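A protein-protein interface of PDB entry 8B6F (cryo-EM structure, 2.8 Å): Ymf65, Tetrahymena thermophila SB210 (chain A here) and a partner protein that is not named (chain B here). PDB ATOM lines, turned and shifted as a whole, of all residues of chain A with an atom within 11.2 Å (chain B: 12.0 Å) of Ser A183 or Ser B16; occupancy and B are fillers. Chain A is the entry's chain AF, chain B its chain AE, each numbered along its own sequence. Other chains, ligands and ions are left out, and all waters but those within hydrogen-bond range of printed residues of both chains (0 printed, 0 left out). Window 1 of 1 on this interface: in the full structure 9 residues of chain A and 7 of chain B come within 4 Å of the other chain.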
ATOM      1  N   ASN A 176      31.941  -9.827  20.442  1.00  0.00           N
ATOM      2  CA  ASN A 176      31.347 -10.885  19.632  1.00  0.00           C
ATOM      3  C   ASN A 176      29.957 -11.194  20.177  1.00  0.00           C
ATOM      4  O   ASN A 176      29.819 -11.703  21.294  1.00  0.00           O
ATOM      5  CB  ASN A 176      32.229 -12.129  19.645  1.00  0.00           C
ATOM      6  CG  ASN A 176      31.613 -13.287  18.886  1.00  0.00           C
ATOM      7  OD1 ASN A 176      31.813 -13.431  17.682  1.00  0.00           O
ATOM      8  ND2 ASN A 176      30.859 -14.119  19.590  1.00  0.00           N
ATOM      9  N   LYS A 178      27.696 -13.166  18.497  1.00  0.00           N
ATOM     10  CA  LYS A 178      27.185 -14.251  17.672  1.00  0.00           C
ATOM     11  C   LYS A 178      27.006 -15.562  18.425  1.00  0.00           C
ATOM     12  O   LYS A 178      26.301 -16.446  17.929  1.00  0.00           O
ATOM     13  CB  LYS A 178      28.120 -14.488  16.480  1.00  0.00           C
ATOM     14  CG  LYS A 178      28.227 -13.299  15.538  1.00  0.00           C
ATOM     15  CD  LYS A 178      29.204 -13.558  14.405  1.00  0.00           C
ATOM     16  CE  LYS A 178      30.641 -13.582  14.894  1.00  0.00           C
ATOM     17  NZ  LYS A 178      31.599 -13.806  13.777  1.00  0.00           N
ATOM     18  N   ASP A 179      27.615 -15.710  19.601  1.00  0.00           N
ATOM     19  CA  ASP A 179      27.616 -16.968  20.337  1.00  0.00           C
ATOM     20  C   ASP A 179      26.747 -16.905  21.590  1.00  0.00           C
ATOM     21  O   ASP A 179      26.988 -17.635  22.554  1.00  0.00           O
ATOM     22  CB  ASP A 179      29.044 -17.357  20.709  1.00  0.00           C
ATOM     23  CG  ASP A 179      29.946 -17.477  19.500  1.00  0.00           C
ATOM     24  OD1 ASP A 179      29.432 -17.406  18.365  1.00  0.00           O
ATOM     25  OD2 ASP A 179      31.171 -17.634  19.682  1.00  0.00           O
ATOM     26  N   ASN A 180      25.729 -16.044  21.591  1.00  0.00           N
ATOM     27  CA  ASN A 180      24.886 -15.910  22.774  1.00  0.00           C
ATOM     28  C   ASN A 180      24.126 -17.198  23.058  1.00  0.00           C
ATOM     29  O   ASN A 180      23.967 -17.589  24.220  1.00  0.00           O
ATOM     30  CB  ASN A 180      23.912 -14.744  22.598  1.00  0.00           C
ATOM     31  CG  ASN A 180      24.595 -13.396  22.695  1.00  0.00           C
ATOM     32  OD1 ASN A 180      25.646 -13.263  23.316  1.00  0.00           O
ATOM     33  ND2 ASN A 180      23.994 -12.385  22.080  1.00  0.00           N
ATOM     34  N   TYR A 181      23.644 -17.868  22.013  1.00  0.00           N
ATOM     35  CA  TYR A 181      22.792 -19.041  22.156  1.00  0.00           C
ATOM     36  C   TYR A 181      23.419 -20.267  21.499  1.00  0.00           C
ATOM     37  O   TYR A 181      22.718 -21.110  20.938  1.00  0.00           O
ATOM     38  CB  TYR A 181      21.407 -18.765  21.572  1.00  0.00           C
ATOM     39  CG  TYR A 181      20.836 -17.437  22.006  1.00  0.00           C
ATOM     40  CD1 TYR A 181      20.370 -17.250  23.300  1.00  0.00           C
ATOM     41  CD2 TYR A 181      20.769 -16.370  21.124  1.00  0.00           C
ATOM     42  CE1 TYR A 181      19.852 -16.034  23.702  1.00  0.00           C
ATOM     43  CE2 TYR A 181      20.254 -15.153  21.515  1.00  0.00           C
ATOM     44  CZ  TYR A 181      19.796 -14.990  22.805  1.00  0.00           C
ATOM     45  OH  TYR A 181      19.282 -13.777  23.195  1.00  0.00           O
ATOM     46  N   PHE A 182      24.743 -20.371  21.559  1.00  0.00           N
ATOM     47  CA  PHE A 182      25.461 -21.530  21.053  1.00  0.00           C
ATOM     48  C   PHE A 182      26.612 -21.845  21.996  1.00  0.00           C
ATOM     49  O   PHE A 182      27.189 -20.947  22.615  1.00  0.00           O
ATOM     50  CB  PHE A 182      25.987 -21.294  19.632  1.00  0.00           C
ATOM     51  CG  PHE A 182      26.450 -22.543  18.943  1.00  0.00           C
ATOM     52  CD1 PHE A 182      25.547 -23.358  18.280  1.00  0.00           C
ATOM     53  CD2 PHE A 182      27.787 -22.899  18.947  1.00  0.00           C
ATOM     54  CE1 PHE A 182      25.967 -24.506  17.642  1.00  0.00           C
ATOM     55  CE2 PHE A 182      28.214 -24.049  18.310  1.00  0.00           C
ATOM     56  CZ  PHE A 182      27.302 -24.852  17.657  1.00  0.00           C
ATOM     57  N   SER A 183      26.936 -23.129  22.104  1.00  0.00           N
ATOM     58  CA  SER A 183      27.982 -23.593  23.006  1.00  0.00           C
ATOM     59  C   SER A 183      29.318 -23.592  22.275  1.00  0.00           C
ATOM     60  O   SER A 183      29.468 -24.252  21.243  1.00  0.00           O
ATOM     61  CB  SER A 183      27.665 -24.992  23.526  1.00  0.00           C
ATOM     62  OG  SER A 183      26.454 -25.001  24.256  1.00  0.00           O
ATOM     63  N   ILE A 184      30.283 -22.851  22.813  1.00  0.00           N
ATOM     64  CA  ILE A 184      31.642 -22.804  22.287  1.00  0.00           C
ATOM     65  C   ILE A 184      32.549 -23.481  23.301  1.00  0.00           C
ATOM     66  O   ILE A 184      32.518 -23.149  24.492  1.00  0.00           O
ATOM     67  CB  ILE A 184      32.097 -21.360  22.019  1.00  0.00           C
ATOM     68  CG1 ILE A 184      31.071 -20.619  21.161  1.00  0.00           C
ATOM     69  CG2 ILE A 184      33.462 -21.350  21.348  1.00  0.00           C
ATOM     70  CD1 ILE A 184      30.795 -21.262  19.821  1.00  0.00           C
ATOM     71  N   PHE A 185      33.357 -24.425  22.832  1.00  0.00           N
ATOM     72  CA  PHE A 185      34.200 -25.236  23.697  1.00  0.00           C
ATOM     73  C   PHE A 185      35.642 -24.757  23.592  1.00  0.00           C
ATOM     74  O   PHE A 185      36.203 -24.694  22.494  1.00  0.00           O
ATOM     75  CB  PHE A 185      34.092 -26.710  23.322  1.00  0.00           C
ATOM     76  CG  PHE A 185      32.683 -27.203  23.216  1.00  0.00           C
ATOM     77  CD1 PHE A 185      31.920 -27.406  24.352  1.00  0.00           C
ATOM     78  CD2 PHE A 185      32.122 -27.466  21.980  1.00  0.00           C
ATOM     79  CE1 PHE A 185      30.621 -27.859  24.256  1.00  0.00           C
ATOM     80  CE2 PHE A 185      30.826 -27.917  21.877  1.00  0.00           C
ATOM     81  CZ  PHE A 185      30.074 -28.116  23.015  1.00  0.00           C
ATOM     82  N   SER A 186      36.233 -24.420  24.735  1.00  0.00           N
ATOM     83  CA  SER A 186      37.628 -24.010  24.827  1.00  0.00           C
ATOM     84  C   SER A 186      38.307 -24.878  25.873  1.00  0.00           C
ATOM     85  O   SER A 186      37.866 -24.920  27.025  1.00  0.00           O
ATOM     86  CB  SER A 186      37.743 -22.528  25.194  1.00  0.00           C
ATOM     87  OG  SER A 186      39.097 -22.131  25.302  1.00  0.00           O
ATOM     88  N   LYS A 187      39.376 -25.567  25.476  1.00  0.00           N
ATOM     89  CA  LYS A 187      40.056 -26.524  26.337  1.00  0.00           C
ATOM     90  C   LYS A 187      41.358 -25.988  26.913  1.00  0.00           C
ATOM     91  O   LYS A 187      42.102 -26.746  27.542  1.00  0.00           O
ATOM     92  CB  LYS A 187      40.341 -27.819  25.577  1.00  0.00           C
ATOM     93  CG  LYS A 187      39.144 -28.731  25.407  1.00  0.00           C
ATOM     94  CD  LYS A 187      38.186 -28.233  24.349  1.00  0.00           C
ATOM     95  CE  LYS A 187      37.065 -29.233  24.134  1.00  0.00           C
ATOM     96  NZ  LYS A 187      36.314 -28.937  22.893  1.00  0.00           N
ATOM     97  N   LYS B  10      20.865 -22.365  39.403  1.00  0.00           N
ATOM     98  CA  LYS B  10      21.495 -22.668  38.118  1.00  0.00           C
ATOM     99  C   LYS B  10      20.448 -22.534  37.018  1.00  0.00           C
ATOM    100  O   LYS B  10      19.652 -23.460  36.799  1.00  0.00           O
ATOM    101  CB  LYS B  10      22.105 -24.067  38.113  1.00  0.00           C
ATOM    102  CG  LYS B  10      22.638 -24.491  36.754  1.00  0.00           C
ATOM    103  CD  LYS B  10      23.346 -25.831  36.816  1.00  0.00           C
ATOM    104  CE  LYS B  10      23.799 -26.267  35.432  1.00  0.00           C
ATOM    105  NZ  LYS B  10      24.459 -27.600  35.444  1.00  0.00           N
ATOM    106  N   PRO B  11      20.417 -21.412  36.306  1.00  0.00           N
ATOM    107  CA  PRO B  11      19.445 -21.249  35.223  1.00  0.00           C
ATOM    108  C   PRO B  11      19.864 -22.020  33.978  1.00  0.00           C
ATOM    109  O   PRO B  11      20.983 -22.517  33.861  1.00  0.00           O
ATOM    110  CB  PRO B  11      19.452 -19.740  34.970  1.00  0.00           C
ATOM    111  CG  PRO B  11      20.821 -19.324  35.329  1.00  0.00           C
ATOM    112  CD  PRO B  11      21.245 -20.204  36.476  1.00  0.00           C
ATOM    113  N   GLU B  12      18.927 -22.112  33.039  1.00  0.00           N
ATOM    114  CA  GLU B  12      19.140 -22.795  31.771  1.00  0.00           C
ATOM    115  C   GLU B  12      19.055 -21.788  30.635  1.00  0.00           C
ATOM    116  O   GLU B  12      18.058 -21.073  30.508  1.00  0.00           O
ATOM    117  CB  GLU B  12      18.114 -23.911  31.571  1.00  0.00           C
ATOM    118  CG  GLU B  12      18.225 -24.612  30.229  1.00  0.00           C
ATOM    119  CD  GLU B  12      17.407 -25.884  30.168  1.00  0.00           C
ATOM    120  OE1 GLU B  12      16.841 -26.276  31.210  1.00  0.00           O
ATOM    121  OE2 GLU B  12      17.331 -26.494  29.082  1.00  0.00           O
ATOM    122  N   SER B  13      20.107 -21.739  29.806  1.00  0.00           N
ATOM    123  CA  SER B  13      20.163 -20.849  28.661  1.00  0.00           C
ATOM    124  C   SER B  13      19.898 -21.623  27.373  1.00  0.00           C
ATOM    125  O   SER B  13      20.196 -22.818  27.292  1.00  0.00           O
ATOM    126  CB  SER B  13      21.534 -20.170  28.574  1.00  0.00           C
ATOM    127  OG  SER B  13      21.621 -19.314  27.449  1.00  0.00           O
ATOM    128  N   PRO B  14      19.339 -20.984  26.347  1.00  0.00           N
ATOM    129  CA  PRO B  14      19.034 -21.716  25.109  1.00  0.00           C
ATOM    130  C   PRO B  14      20.282 -22.333  24.496  1.00  0.00           C
ATOM    131  O   PRO B  14      21.289 -21.655  24.276  1.00  0.00           O
ATOM    132  CB  PRO B  14      18.429 -20.639  24.200  1.00  0.00           C
ATOM    133  CG  PRO B  14      17.936 -19.589  25.121  1.00  0.00           C
ATOM    134  CD  PRO B  14      18.882 -19.584  26.279  1.00  0.00           C
ATOM    135  N   ARG B  15      20.207 -23.634  24.223  1.00  0.00           N
ATOM    136  CA  ARG B  15      21.256 -24.347  23.494  1.00  0.00           C
ATOM    137  C   ARG B  15      22.626 -24.127  24.133  1.00  0.00           C
ATOM    138  O   ARG B  15      23.625 -23.899  23.449  1.00  0.00           O
ATOM    139  CB  ARG B  15      21.268 -23.925  22.024  1.00  0.00           C
ATOM    140  CG  ARG B  15      22.029 -24.873  21.117  1.00  0.00           C
ATOM    141  CD  ARG B  15      22.251 -24.278  19.738  1.00  0.00           C
ATOM    142  NE  ARG B  15      21.009 -24.108  18.991  1.00  0.00           N
ATOM    143  CZ  ARG B  15      20.280 -23.001  18.972  1.00  0.00           C
ATOM    144  NH1 ARG B  15      20.624 -21.932  19.671  1.00  0.00           N
ATOM    145  NH2 ARG B  15      19.177 -22.964  18.232  1.00  0.00           N
ATOM    146  N   SER B  16      22.673 -24.194  25.460  1.00  0.00           N
ATOM    147  CA  SER B  16      23.905 -24.024  26.220  1.00  0.00           C
ATOM    148  C   SER B  16      24.162 -25.272  27.052  1.00  0.00           C
ATOM    149  O   SER B  16      23.283 -25.716  27.796  1.00  0.00           O
ATOM    150  CB  SER B  16      23.824 -22.794  27.126  1.00  0.00           C
ATOM    151  OG  SER B  16      25.017 -22.630  27.870  1.00  0.00           O
ATOM    152  N   ASN B  17      25.364 -25.835  26.923  1.00  0.00           N
ATOM    153  CA  ASN B  17      25.694 -27.047  27.667  1.00  0.00           C
ATOM    154  C   ASN B  17      25.901 -26.756  29.148  1.00  0.00           C
ATOM    155  O   ASN B  17      25.403 -27.494  30.005  1.00  0.00           O
ATOM    156  CB  ASN B  17      26.938 -27.708  27.077  1.00  0.00           C
ATOM    157  CG  ASN B  17      26.689 -28.299  25.705  1.00  0.00           C
ATOM    158  OD1 ASN B  17      25.794 -27.867  24.981  1.00  0.00           O
ATOM    159  ND2 ASN B  17      27.477 -29.304  25.344  1.00  0.00           N
ATOM    160  N   VAL B  18      26.640 -25.693  29.471  1.00  0.00           N
ATOM    161  CA  VAL B  18      26.921 -25.386  30.871  1.00  0.00           C
ATOM    162  C   VAL B  18      25.635 -25.034  31.608  1.00  0.00           C
ATOM    163  O   VAL B  18      25.412 -25.474  32.742  1.00  0.00           O
ATOM    164  CB  VAL B  18      27.972 -24.265  30.979  1.00  0.00           C
ATOM    165  CG1 VAL B  18      29.275 -24.700  30.339  1.00  0.00           C
ATOM    166  CG2 VAL B  18      27.473 -22.977  30.338  1.00  0.00           C
ATOM    167  N   ASN B  19      24.774 -24.233  30.984  1.00  0.00           N
ATOM    168  CA  ASN B  19      23.476 -23.883  31.560  1.00  0.00           C
ATOM    169  C   ASN B  19      22.433 -24.901  31.100  1.00  0.00           C
ATOM    170  O   ASN B  19      21.555 -24.627  30.282  1.00  0.00           O
ATOM    171  CB  ASN B  19      23.082 -22.464  31.171  1.00  0.00           C
ATOM    172  CG  ASN B  19      24.025 -21.422  31.731  1.00  0.00           C
ATOM    173  OD1 ASN B  19      24.966 -20.998  31.063  1.00  0.00           O
ATOM    174  ND2 ASN B  19      23.778 -21.004  32.965  1.00  0.00           N
ATOM    175  N   SER B  20      22.553 -26.108  31.644  1.00  0.00           N
ATOM    176  CA  SER B  20      21.673 -27.204  31.261  1.00  0.00           C
ATOM    177  C   SER B  20      21.844 -28.333  32.264  1.00  0.00           C
ATOM    178  O   SER B  20      22.731 -28.302  33.120  1.00  0.00           O
ATOM    179  CB  SER B  20      21.976 -27.686  29.839  1.00  0.00           C
ATOM    180  OG  SER B  20      21.226 -28.844  29.520  1.00  0.00           O
ATOM    181  N   LYS B  21      20.975 -29.336  32.148  1.00  0.00           N
ATOM    182  CA  LYS B  21      21.084 -30.530  32.973  1.00  0.00           C
ATOM    183  C   LYS B  21      22.245 -31.387  32.493  1.00  0.00           C
ATOM    184  O   LYS B  21      22.088 -32.197  31.573  1.00  0.00           O
ATOM    185  CB  LYS B  21      19.786 -31.339  32.941  1.00  0.00           C
ATOM    186  CG  LYS B  21      18.572 -30.607  33.485  1.00  0.00           C
ATOM    187  CD  LYS B  21      18.728 -30.283  34.960  1.00  0.00           C
ATOM    188  CE  LYS B  21      17.459 -29.666  35.518  1.00  0.00           C
ATOM    189  NZ  LYS B  21      17.631 -29.257  36.936  1.00  0.00           N
ATOM    190  N   GLN B  22      23.413 -31.214  33.100  1.00  0.00           N
ATOM    191  CA  GLN B  22      24.591 -31.987  32.740  1.00  0.00           C
ATOM    192  C   GLN B  22      24.625 -33.352  33.412  1.00  0.00           C
ATOM    193  O   GLN B  22      25.653 -34.034  33.349  1.00  0.00           O
ATOM    194  CB  GLN B  22      25.855 -31.199  33.091  1.00  0.00           C
ATOM    195  CG  GLN B  22      26.046 -29.950  32.249  1.00  0.00           C
ATOM    196  CD  GLN B  22      27.171 -29.076  32.757  1.00  0.00           C
ATOM    197  OE1 GLN B  22      27.296 -28.845  33.958  1.00  0.00           O
ATOM    198  NE2 GLN B  22      28.006 -28.594  31.846  1.00  0.00           N
ATOM    199  N   ILE B  23      23.527 -33.765  34.044  1.00  0.00           N
ATOM    200  CA  ILE B  23      23.464 -35.010  34.792  1.00  0.00           C
ATOM    201  C   ILE B  23      22.174 -35.730  34.432  1.00  0.00           C
ATOM    202  O   ILE B  23      21.192 -35.118  34.005  1.00  0.00           O
ATOM    203  CB  ILE B  23      23.540 -34.763  36.315  1.00  0.00           C
ATOM    204  CG1 ILE B  23      23.585 -36.088  37.073  1.00  0.00           C
ATOM    205  CG2 ILE B  23      22.355 -33.919  36.774  1.00  0.00           C
ATOM    206  CD1 ILE B  23      23.840 -35.940  38.548  1.00  0.00           C
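NE2 of Gln B22 sits at hydrogen-bond distance from O of Asn B17, 3.4 Å away.
NH1 of Arg B15 is in hydrogen-bond range of O of Tyr A181, at 2.6 Å.
O of Arg B15 lies within hydrogen-bond range of OG of Ser A183 (3.1 Å).
OG of Ser A183 is in hydrogen-bond range of N of Asn B17 (3.0 Å).
Among the printed residues, merely in contact across the chains: Ser A183 with Ser B16 (3.4 Å), Phe A185 with Asn B17 (3.6 Å), Tyr A181 with Pro B14 (3.7 Å) and Phe A182 with Arg B15 (3.7 Å).
Asn A180 touches none of the printed residues of chain B.
Of the printed residues of chain B, Tyr A181 touches Pro B14 and Arg B15.
Ser A183 touches three residues of chain B.
Ile A184 touches none of the printed residues of chain B.
Pro B14 touches just one residue of chain A: Tyr A181 (3.7 Å).
Printed residues of chain A within 4 Å of Arg B15: Tyr A181 (2.6 Å), Phe A182 (3.7 Å) and Ser A183 (3.1 Å).
Of chain A, only Ser A183 comes within 4 Å of Ser B16.
Of chain A, only Ser A183 (3.0 Å) and Phe A185 (3.6 Å) come within 4 Å of Asn B17.
No residue of chain A comes within 4 Å of Val B18.
No residue of chain A comes within 4 Å of Asn B19.
No residue of chain A comes within 4 Å of Ser B20.
Lys B21 touches none of the printed residues of chain A.
Of the 11 printed residues of chain A, 4 touch a printed residue of chain B.
Hydrophobic or aromatic side chains of chain A within 4 Å of the printed part of chain B: Tyr A181, Phe A182 and Phe A185.
Among the printed residues, 7 pairs touch across the chains.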
